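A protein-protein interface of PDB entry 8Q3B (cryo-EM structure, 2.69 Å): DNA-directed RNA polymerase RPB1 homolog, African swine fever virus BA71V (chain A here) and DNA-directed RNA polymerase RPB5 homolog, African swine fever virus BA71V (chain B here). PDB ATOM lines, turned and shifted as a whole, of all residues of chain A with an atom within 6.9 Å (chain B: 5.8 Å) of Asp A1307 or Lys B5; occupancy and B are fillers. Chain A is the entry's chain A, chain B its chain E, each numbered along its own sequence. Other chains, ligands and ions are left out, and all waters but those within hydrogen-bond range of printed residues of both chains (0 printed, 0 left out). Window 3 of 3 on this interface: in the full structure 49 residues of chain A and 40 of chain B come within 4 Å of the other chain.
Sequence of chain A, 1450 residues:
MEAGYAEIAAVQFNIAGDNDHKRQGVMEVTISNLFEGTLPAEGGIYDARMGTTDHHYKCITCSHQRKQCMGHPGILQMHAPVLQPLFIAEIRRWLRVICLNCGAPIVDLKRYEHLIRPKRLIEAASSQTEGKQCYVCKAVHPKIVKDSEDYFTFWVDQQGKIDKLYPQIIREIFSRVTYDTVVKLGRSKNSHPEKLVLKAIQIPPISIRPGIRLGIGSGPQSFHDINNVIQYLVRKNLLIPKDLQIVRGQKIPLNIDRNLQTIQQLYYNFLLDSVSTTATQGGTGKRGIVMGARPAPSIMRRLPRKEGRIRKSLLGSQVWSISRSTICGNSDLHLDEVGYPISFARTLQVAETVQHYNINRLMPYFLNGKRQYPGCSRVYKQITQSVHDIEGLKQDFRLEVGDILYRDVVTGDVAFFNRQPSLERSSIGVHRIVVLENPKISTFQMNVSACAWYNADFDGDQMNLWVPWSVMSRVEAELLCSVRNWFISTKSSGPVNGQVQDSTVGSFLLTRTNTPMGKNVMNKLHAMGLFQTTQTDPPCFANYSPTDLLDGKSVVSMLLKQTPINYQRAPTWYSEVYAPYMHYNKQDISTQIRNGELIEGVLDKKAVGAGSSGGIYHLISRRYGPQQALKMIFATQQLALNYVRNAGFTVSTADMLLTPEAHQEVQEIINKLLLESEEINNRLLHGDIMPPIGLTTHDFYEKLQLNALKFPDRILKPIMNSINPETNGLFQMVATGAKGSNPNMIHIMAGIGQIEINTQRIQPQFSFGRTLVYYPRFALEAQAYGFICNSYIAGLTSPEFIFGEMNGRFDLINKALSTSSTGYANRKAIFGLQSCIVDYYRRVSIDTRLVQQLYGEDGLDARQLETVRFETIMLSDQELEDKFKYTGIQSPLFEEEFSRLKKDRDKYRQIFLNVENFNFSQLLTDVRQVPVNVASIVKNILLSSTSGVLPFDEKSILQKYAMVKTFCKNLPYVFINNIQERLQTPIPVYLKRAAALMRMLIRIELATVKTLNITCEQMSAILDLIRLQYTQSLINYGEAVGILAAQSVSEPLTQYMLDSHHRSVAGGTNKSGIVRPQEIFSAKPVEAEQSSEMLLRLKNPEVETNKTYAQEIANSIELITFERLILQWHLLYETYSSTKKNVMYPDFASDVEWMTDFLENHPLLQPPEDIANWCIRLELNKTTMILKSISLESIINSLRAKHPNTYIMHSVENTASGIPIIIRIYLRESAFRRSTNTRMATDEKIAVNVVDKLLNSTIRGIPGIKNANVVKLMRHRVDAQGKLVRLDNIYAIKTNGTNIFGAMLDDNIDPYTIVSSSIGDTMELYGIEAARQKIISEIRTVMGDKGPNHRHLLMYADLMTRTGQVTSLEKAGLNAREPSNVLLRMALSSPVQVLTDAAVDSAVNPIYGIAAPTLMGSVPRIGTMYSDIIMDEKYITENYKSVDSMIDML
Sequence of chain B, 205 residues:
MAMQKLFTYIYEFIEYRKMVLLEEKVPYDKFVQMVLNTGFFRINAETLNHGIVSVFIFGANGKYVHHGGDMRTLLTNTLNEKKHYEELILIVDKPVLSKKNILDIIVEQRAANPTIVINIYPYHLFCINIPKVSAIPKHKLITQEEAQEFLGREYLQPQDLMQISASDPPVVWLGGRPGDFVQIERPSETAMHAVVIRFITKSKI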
ATOM      1  N   LEU A1098     -12.784  14.578 -25.882  1.00  0.00           N
ATOM      2  CA  LEU A1098     -12.898  14.550 -27.330  1.00  0.00           C
ATOM      3  C   LEU A1098     -13.232  13.135 -27.806  1.00  0.00           C
ATOM      4  O   LEU A1098     -13.137  12.155 -27.062  1.00  0.00           O
ATOM      5  CB  LEU A1098     -11.609  15.058 -27.976  1.00  0.00           C
ATOM      6  CG  LEU A1098     -11.158  16.462 -27.557  1.00  0.00           C
ATOM      7  CD1 LEU A1098     -10.276  17.072 -28.630  1.00  0.00           C
ATOM      8  CD2 LEU A1098     -12.333  17.384 -27.259  1.00  0.00           C
ATOM      9  N   LYS A1099     -13.633  13.040 -29.076  1.00  0.00           N
ATOM     10  CA  LYS A1099     -14.274  11.821 -29.563  1.00  0.00           C
ATOM     11  C   LYS A1099     -13.341  10.616 -29.487  1.00  0.00           C
ATOM     12  O   LYS A1099     -13.764   9.528 -29.079  1.00  0.00           O
ATOM     13  CB  LYS A1099     -14.771  12.027 -30.995  1.00  0.00           C
ATOM     14  CG  LYS A1099     -13.751  12.630 -31.945  1.00  0.00           C
ATOM     15  CD  LYS A1099     -14.018  12.206 -33.380  1.00  0.00           C
ATOM     16  CE  LYS A1099     -13.610  13.288 -34.366  1.00  0.00           C
ATOM     17  NZ  LYS A1099     -14.529  14.460 -34.323  1.00  0.00           N
ATOM     18  N   PHE A1301     -27.644  16.148 -22.002  1.00  0.00           N
ATOM     19  CA  PHE A1301     -28.306  15.676 -23.213  1.00  0.00           C
ATOM     20  C   PHE A1301     -27.689  16.308 -24.456  1.00  0.00           C
ATOM     21  O   PHE A1301     -27.373  15.615 -25.433  1.00  0.00           O
ATOM     22  CB  PHE A1301     -29.803  15.983 -23.130  1.00  0.00           C
ATOM     23  CG  PHE A1301     -30.614  15.394 -24.251  1.00  0.00           C
ATOM     24  CD1 PHE A1301     -30.342  14.129 -24.737  1.00  0.00           C
ATOM     25  CD2 PHE A1301     -31.659  16.109 -24.811  1.00  0.00           C
ATOM     26  CE1 PHE A1301     -31.090  13.591 -25.762  1.00  0.00           C
ATOM     27  CE2 PHE A1301     -32.410  15.575 -25.836  1.00  0.00           C
ATOM     28  CZ  PHE A1301     -32.126  14.314 -26.312  1.00  0.00           C
ATOM     29  N   GLY A1302     -27.492  17.627 -24.430  1.00  0.00           N
ATOM     30  CA  GLY A1302     -26.887  18.295 -25.569  1.00  0.00           C
ATOM     31  C   GLY A1302     -25.484  17.797 -25.853  1.00  0.00           C
ATOM     32  O   GLY A1302     -25.102  17.610 -27.011  1.00  0.00           O
ATOM     33  N   ALA A1303     -24.695  17.574 -24.800  1.00  0.00           N
ATOM     34  CA  ALA A1303     -23.354  17.035 -24.987  1.00  0.00           C
ATOM     35  C   ALA A1303     -23.406  15.644 -25.605  1.00  0.00           C
ATOM     36  O   ALA A1303     -22.588  15.310 -26.469  1.00  0.00           O
ATOM     37  CB  ALA A1303     -22.612  17.007 -23.653  1.00  0.00           C
ATOM     38  N   MET A1304     -24.361  14.816 -25.173  1.00  0.00           N
ATOM     39  CA  MET A1304     -24.508  13.493 -25.770  1.00  0.00           C
ATOM     40  C   MET A1304     -24.837  13.595 -27.252  1.00  0.00           C
ATOM     41  O   MET A1304     -24.301  12.836 -28.068  1.00  0.00           O
ATOM     42  CB  MET A1304     -25.592  12.696 -25.044  1.00  0.00           C
ATOM     43  CG  MET A1304     -25.217  12.270 -23.633  1.00  0.00           C
ATOM     44  SD  MET A1304     -26.448  11.244 -22.794  1.00  0.00           S
ATOM     45  CE  MET A1304     -27.907  11.476 -23.808  1.00  0.00           C
ATOM     46  N   LEU A1305     -25.719  14.525 -27.622  1.00  0.00           N
ATOM     47  CA  LEU A1305     -26.094  14.652 -29.028  1.00  0.00           C
ATOM     48  C   LEU A1305     -24.904  15.065 -29.886  1.00  0.00           C
ATOM     49  O   LEU A1305     -24.788  14.639 -31.041  1.00  0.00           O
ATOM     50  CB  LEU A1305     -27.239  15.654 -29.182  1.00  0.00           C
ATOM     51  CG  LEU A1305     -28.557  15.307 -28.486  1.00  0.00           C
ATOM     52  CD1 LEU A1305     -29.657  16.248 -28.946  1.00  0.00           C
ATOM     53  CD2 LEU A1305     -28.956  13.861 -28.736  1.00  0.00           C
ATOM     54  N   ASP A1306     -24.012  15.891 -29.345  1.00  0.00           N
ATOM     55  CA  ASP A1306     -22.870  16.366 -30.118  1.00  0.00           C
ATOM     56  C   ASP A1306     -21.954  15.207 -30.490  1.00  0.00           C
ATOM     57  O   ASP A1306     -21.642  14.350 -29.658  1.00  0.00           O
ATOM     58  CB  ASP A1306     -22.098  17.416 -29.321  1.00  0.00           C
ATOM     59  CG  ASP A1306     -21.059  18.132 -30.157  1.00  0.00           C
ATOM     60  OD1 ASP A1306     -20.951  17.827 -31.364  1.00  0.00           O
ATOM     61  OD2 ASP A1306     -20.351  19.003 -29.612  1.00  0.00           O
ATOM     62  N   ASP A1307     -21.519  15.186 -31.753  1.00  0.00           N
ATOM     63  CA  ASP A1307     -20.681  14.094 -32.239  1.00  0.00           C
ATOM     64  C   ASP A1307     -19.224  14.260 -31.821  1.00  0.00           C
ATOM     65  O   ASP A1307     -18.542  13.268 -31.539  1.00  0.00           O
ATOM     66  CB  ASP A1307     -20.780  14.000 -33.762  1.00  0.00           C
ATOM     67  CG  ASP A1307     -22.081  13.376 -34.223  1.00  0.00           C
ATOM     68  OD1 ASP A1307     -22.380  12.240 -33.798  1.00  0.00           O
ATOM     69  OD2 ASP A1307     -22.805  14.022 -35.010  1.00  0.00           O
ATOM     70  N   ASN A1308     -18.728  15.498 -31.778  1.00  0.00           N
ATOM     71  CA  ASN A1308     -17.318  15.713 -31.465  1.00  0.00           C
ATOM     72  C   ASN A1308     -16.978  15.264 -30.051  1.00  0.00           C
ATOM     73  O   ASN A1308     -15.839  14.866 -29.785  1.00  0.00           O
ATOM     74  CB  ASN A1308     -16.959  17.187 -31.649  1.00  0.00           C
ATOM     75  CG  ASN A1308     -17.179  17.667 -33.068  1.00  0.00           C
ATOM     76  OD1 ASN A1308     -16.612  17.123 -34.014  1.00  0.00           O
ATOM     77  ND2 ASN A1308     -18.007  18.694 -33.223  1.00  0.00           N
ATOM     78  N   ILE A1309     -17.940  15.323 -29.139  1.00  0.00           N
ATOM     79  CA  ILE A1309     -17.716  14.978 -27.742  1.00  0.00           C
ATOM     80  C   ILE A1309     -17.979  13.492 -27.546  1.00  0.00           C
ATOM     81  O   ILE A1309     -18.971  12.955 -28.055  1.00  0.00           O
ATOM     82  CB  ILE A1309     -18.616  15.819 -26.821  1.00  0.00           C
ATOM     83  CG1 ILE A1309     -18.329  17.314 -27.001  1.00  0.00           C
ATOM     84  CG2 ILE A1309     -18.426  15.405 -25.373  1.00  0.00           C
ATOM     85  CD1 ILE A1309     -16.874  17.700 -26.829  1.00  0.00           C
ATOM     86  N   ASP A1310     -17.097  12.830 -26.812  1.00  0.00           N
ATOM     87  CA  ASP A1310     -17.309  11.431 -26.463  1.00  0.00           C
ATOM     88  C   ASP A1310     -18.484  11.333 -25.497  1.00  0.00           C
ATOM     89  O   ASP A1310     -18.459  11.981 -24.443  1.00  0.00           O
ATOM     90  CB  ASP A1310     -16.049  10.844 -25.837  1.00  0.00           C
ATOM     91  CG  ASP A1310     -16.244   9.419 -25.363  1.00  0.00           C
ATOM     92  OD1 ASP A1310     -16.566   8.551 -26.201  1.00  0.00           O
ATOM     93  OD2 ASP A1310     -16.069   9.165 -24.154  1.00  0.00           O
ATOM     94  N   PRO A1311     -19.522  10.546 -25.799  1.00  0.00           N
ATOM     95  CA  PRO A1311     -20.740  10.592 -24.980  1.00  0.00           C
ATOM     96  C   PRO A1311     -20.707   9.717 -23.739  1.00  0.00           C
ATOM     97  O   PRO A1311     -21.575   9.883 -22.871  1.00  0.00           O
ATOM     98  CB  PRO A1311     -21.815  10.107 -25.956  1.00  0.00           C
ATOM     99  CG  PRO A1311     -21.096   9.122 -26.808  1.00  0.00           C
ATOM    100  CD  PRO A1311     -19.668   9.614 -26.931  1.00  0.00           C
ATOM    101  N   MET B   1     -28.199  15.384 -33.359  1.00  0.00           N
ATOM    102  CA  MET B   1     -29.682  15.444 -33.495  1.00  0.00           C
ATOM    103  C   MET B   1     -30.300  14.265 -32.753  1.00  0.00           C
ATOM    104  O   MET B   1     -29.816  13.137 -32.852  1.00  0.00           O
ATOM    105  CB  MET B   1     -30.085  15.433 -34.974  1.00  0.00           C
ATOM    106  CG  MET B   1     -31.572  15.223 -35.240  1.00  0.00           C
ATOM    107  SD  MET B   1     -32.577  16.611 -34.678  1.00  0.00           S
ATOM    108  CE  MET B   1     -34.201  15.861 -34.603  1.00  0.00           C
ATOM    109  N   ALA B   2     -31.375  14.531 -32.007  1.00  0.00           N
ATOM    110  CA  ALA B   2     -32.008  13.472 -31.229  1.00  0.00           C
ATOM    111  C   ALA B   2     -32.503  12.349 -32.130  1.00  0.00           C
ATOM    112  O   ALA B   2     -32.344  11.167 -31.806  1.00  0.00           O
ATOM    113  CB  ALA B   2     -33.158  14.043 -30.402  1.00  0.00           C
ATOM    114  N   MET B   3     -33.100  12.699 -33.271  1.00  0.00           N
ATOM    115  CA  MET B   3     -33.630  11.680 -34.171  1.00  0.00           C
ATOM    116  C   MET B   3     -32.531  10.744 -34.652  1.00  0.00           C
ATOM    117  O   MET B   3     -32.732   9.527 -34.722  1.00  0.00           O
ATOM    118  CB  MET B   3     -34.324  12.346 -35.361  1.00  0.00           C
ATOM    119  CG  MET B   3     -35.797  12.722 -35.153  1.00  0.00           C
ATOM    120  SD  MET B   3     -36.769  11.586 -34.140  1.00  0.00           S
ATOM    121  CE  MET B   3     -37.587  12.732 -33.034  1.00  0.00           C
ATOM    122  N   GLN B   4     -31.362  11.288 -34.996  1.00  0.00           N
ATOM    123  CA  GLN B   4     -30.254  10.438 -35.421  1.00  0.00           C
ATOM    124  C   GLN B   4     -29.847   9.480 -34.307  1.00  0.00           C
ATOM    125  O   GLN B   4     -29.738   8.266 -34.520  1.00  0.00           O
ATOM    126  CB  GLN B   4     -29.066  11.302 -35.845  1.00  0.00           C
ATOM    127  CG  GLN B   4     -28.562  11.035 -37.257  1.00  0.00           C
ATOM    128  CD  GLN B   4     -28.090   9.608 -37.457  1.00  0.00           C
ATOM    129  OE1 GLN B   4     -28.122   8.794 -36.537  1.00  0.00           O
ATOM    130  NE2 GLN B   4     -27.648   9.298 -38.671  1.00  0.00           N
ATOM    131  N   LYS B   5     -29.622  10.012 -33.104  1.00  0.00           N
ATOM    132  CA  LYS B   5     -29.221   9.167 -31.985  1.00  0.00           C
ATOM    133  C   LYS B   5     -30.326   8.189 -31.610  1.00  0.00           C
ATOM    134  O   LYS B   5     -30.052   7.026 -31.292  1.00  0.00           O
ATOM    135  CB  LYS B   5     -28.840  10.034 -30.786  1.00  0.00           C
ATOM    136  CG  LYS B   5     -27.697  10.996 -31.058  1.00  0.00           C
ATOM    137  CD  LYS B   5     -26.416  10.254 -31.405  1.00  0.00           C
ATOM    138  CE  LYS B   5     -25.226  11.193 -31.463  1.00  0.00           C
ATOM    139  NZ  LYS B   5     -23.947  10.455 -31.652  1.00  0.00           N
ATOM    140  N   LEU B   6     -31.580   8.643 -31.626  1.00  0.00           N
ATOM    141  CA  LEU B   6     -32.687   7.744 -31.317  1.00  0.00           C
ATOM    142  C   LEU B   6     -32.729   6.586 -32.300  1.00  0.00           C
ATOM    143  O   LEU B   6     -32.876   5.425 -31.905  1.00  0.00           O
ATOM    144  CB  LEU B   6     -34.012   8.508 -31.337  1.00  0.00           C
ATOM    145  CG  LEU B   6     -34.753   8.631 -30.006  1.00  0.00           C
ATOM    146  CD1 LEU B   6     -36.010   9.457 -30.193  1.00  0.00           C
ATOM    147  CD2 LEU B   6     -35.102   7.263 -29.445  1.00  0.00           C
ATOM    148  N   PHE B   7     -32.590   6.882 -33.592  1.00  0.00           N
ATOM    149  CA  PHE B   7     -32.598   5.823 -34.593  1.00  0.00           C
ATOM    150  C   PHE B   7     -31.428   4.873 -34.389  1.00  0.00           C
ATOM    151  O   PHE B   7     -31.577   3.653 -34.514  1.00  0.00           O
ATOM    152  CB  PHE B   7     -32.555   6.429 -35.994  1.00  0.00           C
ATOM    153  CG  PHE B   7     -33.001   5.487 -37.071  1.00  0.00           C
ATOM    154  CD1 PHE B   7     -34.281   4.964 -37.059  1.00  0.00           C
ATOM    155  CD2 PHE B   7     -32.138   5.117 -38.086  1.00  0.00           C
ATOM    156  CE1 PHE B   7     -34.695   4.096 -38.043  1.00  0.00           C
ATOM    157  CE2 PHE B   7     -32.548   4.247 -39.073  1.00  0.00           C
ATOM    158  CZ  PHE B   7     -33.829   3.736 -39.049  1.00  0.00           C
ATOM    159  N   THR B   8     -30.251   5.417 -34.076  1.00  0.00           N
ATOM    160  CA  THR B   8     -29.076   4.570 -33.896  1.00  0.00           C
ATOM    161  C   THR B   8     -29.234   3.644 -32.697  1.00  0.00           C
ATOM    162  O   THR B   8     -28.854   2.469 -32.758  1.00  0.00           O
ATOM    163  CB  THR B   8     -27.827   5.436 -33.734  1.00  0.00           C
ATOM    164  OG1 THR B   8     -27.732   6.355 -34.828  1.00  0.00           O
ATOM    165  CG2 THR B   8     -26.575   4.570 -33.694  1.00  0.00           C
ATOM    166  N   TYR B   9     -29.792   4.150 -31.596  1.00  0.00           N
ATOM    167  CA  TYR B   9     -29.721   3.454 -30.319  1.00  0.00           C
ATOM    168  C   TYR B   9     -31.007   2.743 -29.915  1.00  0.00           C
ATOM    169  O   TYR B   9     -30.976   1.950 -28.971  1.00  0.00           O
ATOM    170  CB  TYR B   9     -29.324   4.438 -29.214  1.00  0.00           C
ATOM    171  CG  TYR B   9     -27.889   4.899 -29.314  1.00  0.00           C
ATOM    172  CD1 TYR B   9     -26.841   4.008 -29.133  1.00  0.00           C
ATOM    173  CD2 TYR B   9     -27.581   6.221 -29.596  1.00  0.00           C
ATOM    174  CE1 TYR B   9     -25.528   4.421 -29.228  1.00  0.00           C
ATOM    175  CE2 TYR B   9     -26.271   6.644 -29.692  1.00  0.00           C
ATOM    176  CZ  TYR B   9     -25.249   5.740 -29.508  1.00  0.00           C
ATOM    177  OH  TYR B   9     -23.942   6.156 -29.603  1.00  0.00           O
ATOM    178  N   ILE B  10     -32.129   2.976 -30.597  1.00  0.00           N
ATOM    179  CA  ILE B  10     -33.346   2.260 -30.233  1.00  0.00           C
ATOM    180  C   ILE B  10     -33.206   0.780 -30.561  1.00  0.00           C
ATOM    181  O   ILE B  10     -33.660  -0.086 -29.804  1.00  0.00           O
ATOM    182  CB  ILE B  10     -34.567   2.889 -30.928  1.00  0.00           C
ATOM    183  CG1 ILE B  10     -35.865   2.336 -30.333  1.00  0.00           C
ATOM    184  CG2 ILE B  10     -34.524   2.640 -32.429  1.00  0.00           C
ATOM    185  CD1 ILE B  10     -36.095   2.737 -28.889  1.00  0.00           C
ATOM    186  N   PHE B 126     -33.133   6.792 -24.683  1.00  0.00           N
ATOM    187  CA  PHE B 126     -32.766   5.955 -25.817  1.00  0.00           C
ATOM    188  C   PHE B 126     -31.836   6.662 -26.798  1.00  0.00           C
ATOM    189  O   PHE B 126     -31.675   6.200 -27.931  1.00  0.00           O
ATOM    190  CB  PHE B 126     -34.022   5.472 -26.538  1.00  0.00           C
ATOM    191  CG  PHE B 126     -35.007   4.783 -25.640  1.00  0.00           C
ATOM    192  CD1 PHE B 126     -35.943   5.511 -24.929  1.00  0.00           C
ATOM    193  CD2 PHE B 126     -34.996   3.406 -25.508  1.00  0.00           C
ATOM    194  CE1 PHE B 126     -36.848   4.879 -24.103  1.00  0.00           C
ATOM    195  CE2 PHE B 126     -35.899   2.770 -24.683  1.00  0.00           C
ATOM    196  CZ  PHE B 126     -36.825   3.507 -23.980  1.00  0.00           C
ATOM    197  N   CYS B 127     -31.220   7.769 -26.391  1.00  0.00           N
ATOM    198  CA  CYS B 127     -30.287   8.498 -27.238  1.00  0.00           C
ATOM    199  C   CYS B 127     -28.836   8.115 -26.977  1.00  0.00           C
ATOM    200  O   CYS B 127     -27.930   8.742 -27.534  1.00  0.00           O
ATOM    201  CB  CYS B 127     -30.472  10.004 -27.050  1.00  0.00           C
ATOM    202  SG  CYS B 127     -31.952  10.659 -27.850  1.00  0.00           S
ATOM    203  N   ILE B 128     -28.595   7.105 -26.141  1.00  0.00           N
ATOM    204  CA  ILE B 128     -27.242   6.647 -25.846  1.00  0.00           C
ATOM    205  C   ILE B 128     -27.334   5.211 -25.361  1.00  0.00           C
ATOM    206  O   ILE B 128     -28.375   4.768 -24.876  1.00  0.00           O
ATOM    207  CB  ILE B 128     -26.556   7.556 -24.794  1.00  0.00           C
ATOM    208  CG1 ILE B 128     -25.044   7.323 -24.797  1.00  0.00           C
ATOM    209  CG2 ILE B 128     -27.136   7.305 -23.411  1.00  0.00           C
ATOM    210  CD1 ILE B 128     -24.280   8.274 -23.906  1.00  0.00           C
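The side-chain carboxylate of Asp A1307 is in salt-bridge range of the side-chain amino group of Lys B5 (3.2 Å).
Among the printed residues, pairs that only touch across the chains: Pro A1311 with Ile B128, Leu A1305 with Lys B5, Phe A1301 with Cys B127, Met A1304 with Ile B128, Met A1304 with Lys B5 and Leu A1305 with Ala B2.
Of the printed residues of chain B, Phe A1301 touches Cys B127.
Of chain B, only Lys B5 (3.2 Å) comes within 4 Å of Asp A1307.
Lys B5 touches just these residues of chain A: Met A1304, Leu A1305 and Asp A1307.
Tyr B9 touches none of the printed residues of chain A.
Phe B126 touches none of the printed residues of chain A.
Printed residues of chain A within 4 Å of Ile B128: Met A1304 (3.8 Å) and Pro A1311 (3.3 Å).
Printed residues of chain B that touch a printed residue of chain A: Ala B2, Lys B5, Cys B127 and Ile B128.
Hydrophobic or aromatic side chains of chain B within 4 Å of the printed part of chain A: Ile B128.
Of the 13 printed residues of chain A, 5 touch a printed residue of chain B.
Hydrophobic or aromatic side chains of chain A within 4 Å of the printed part of chain B: Phe A1301, Met A1304, Leu A1305 and Pro A1311.
Among the printed residues, 7 pairs touch across the chains.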
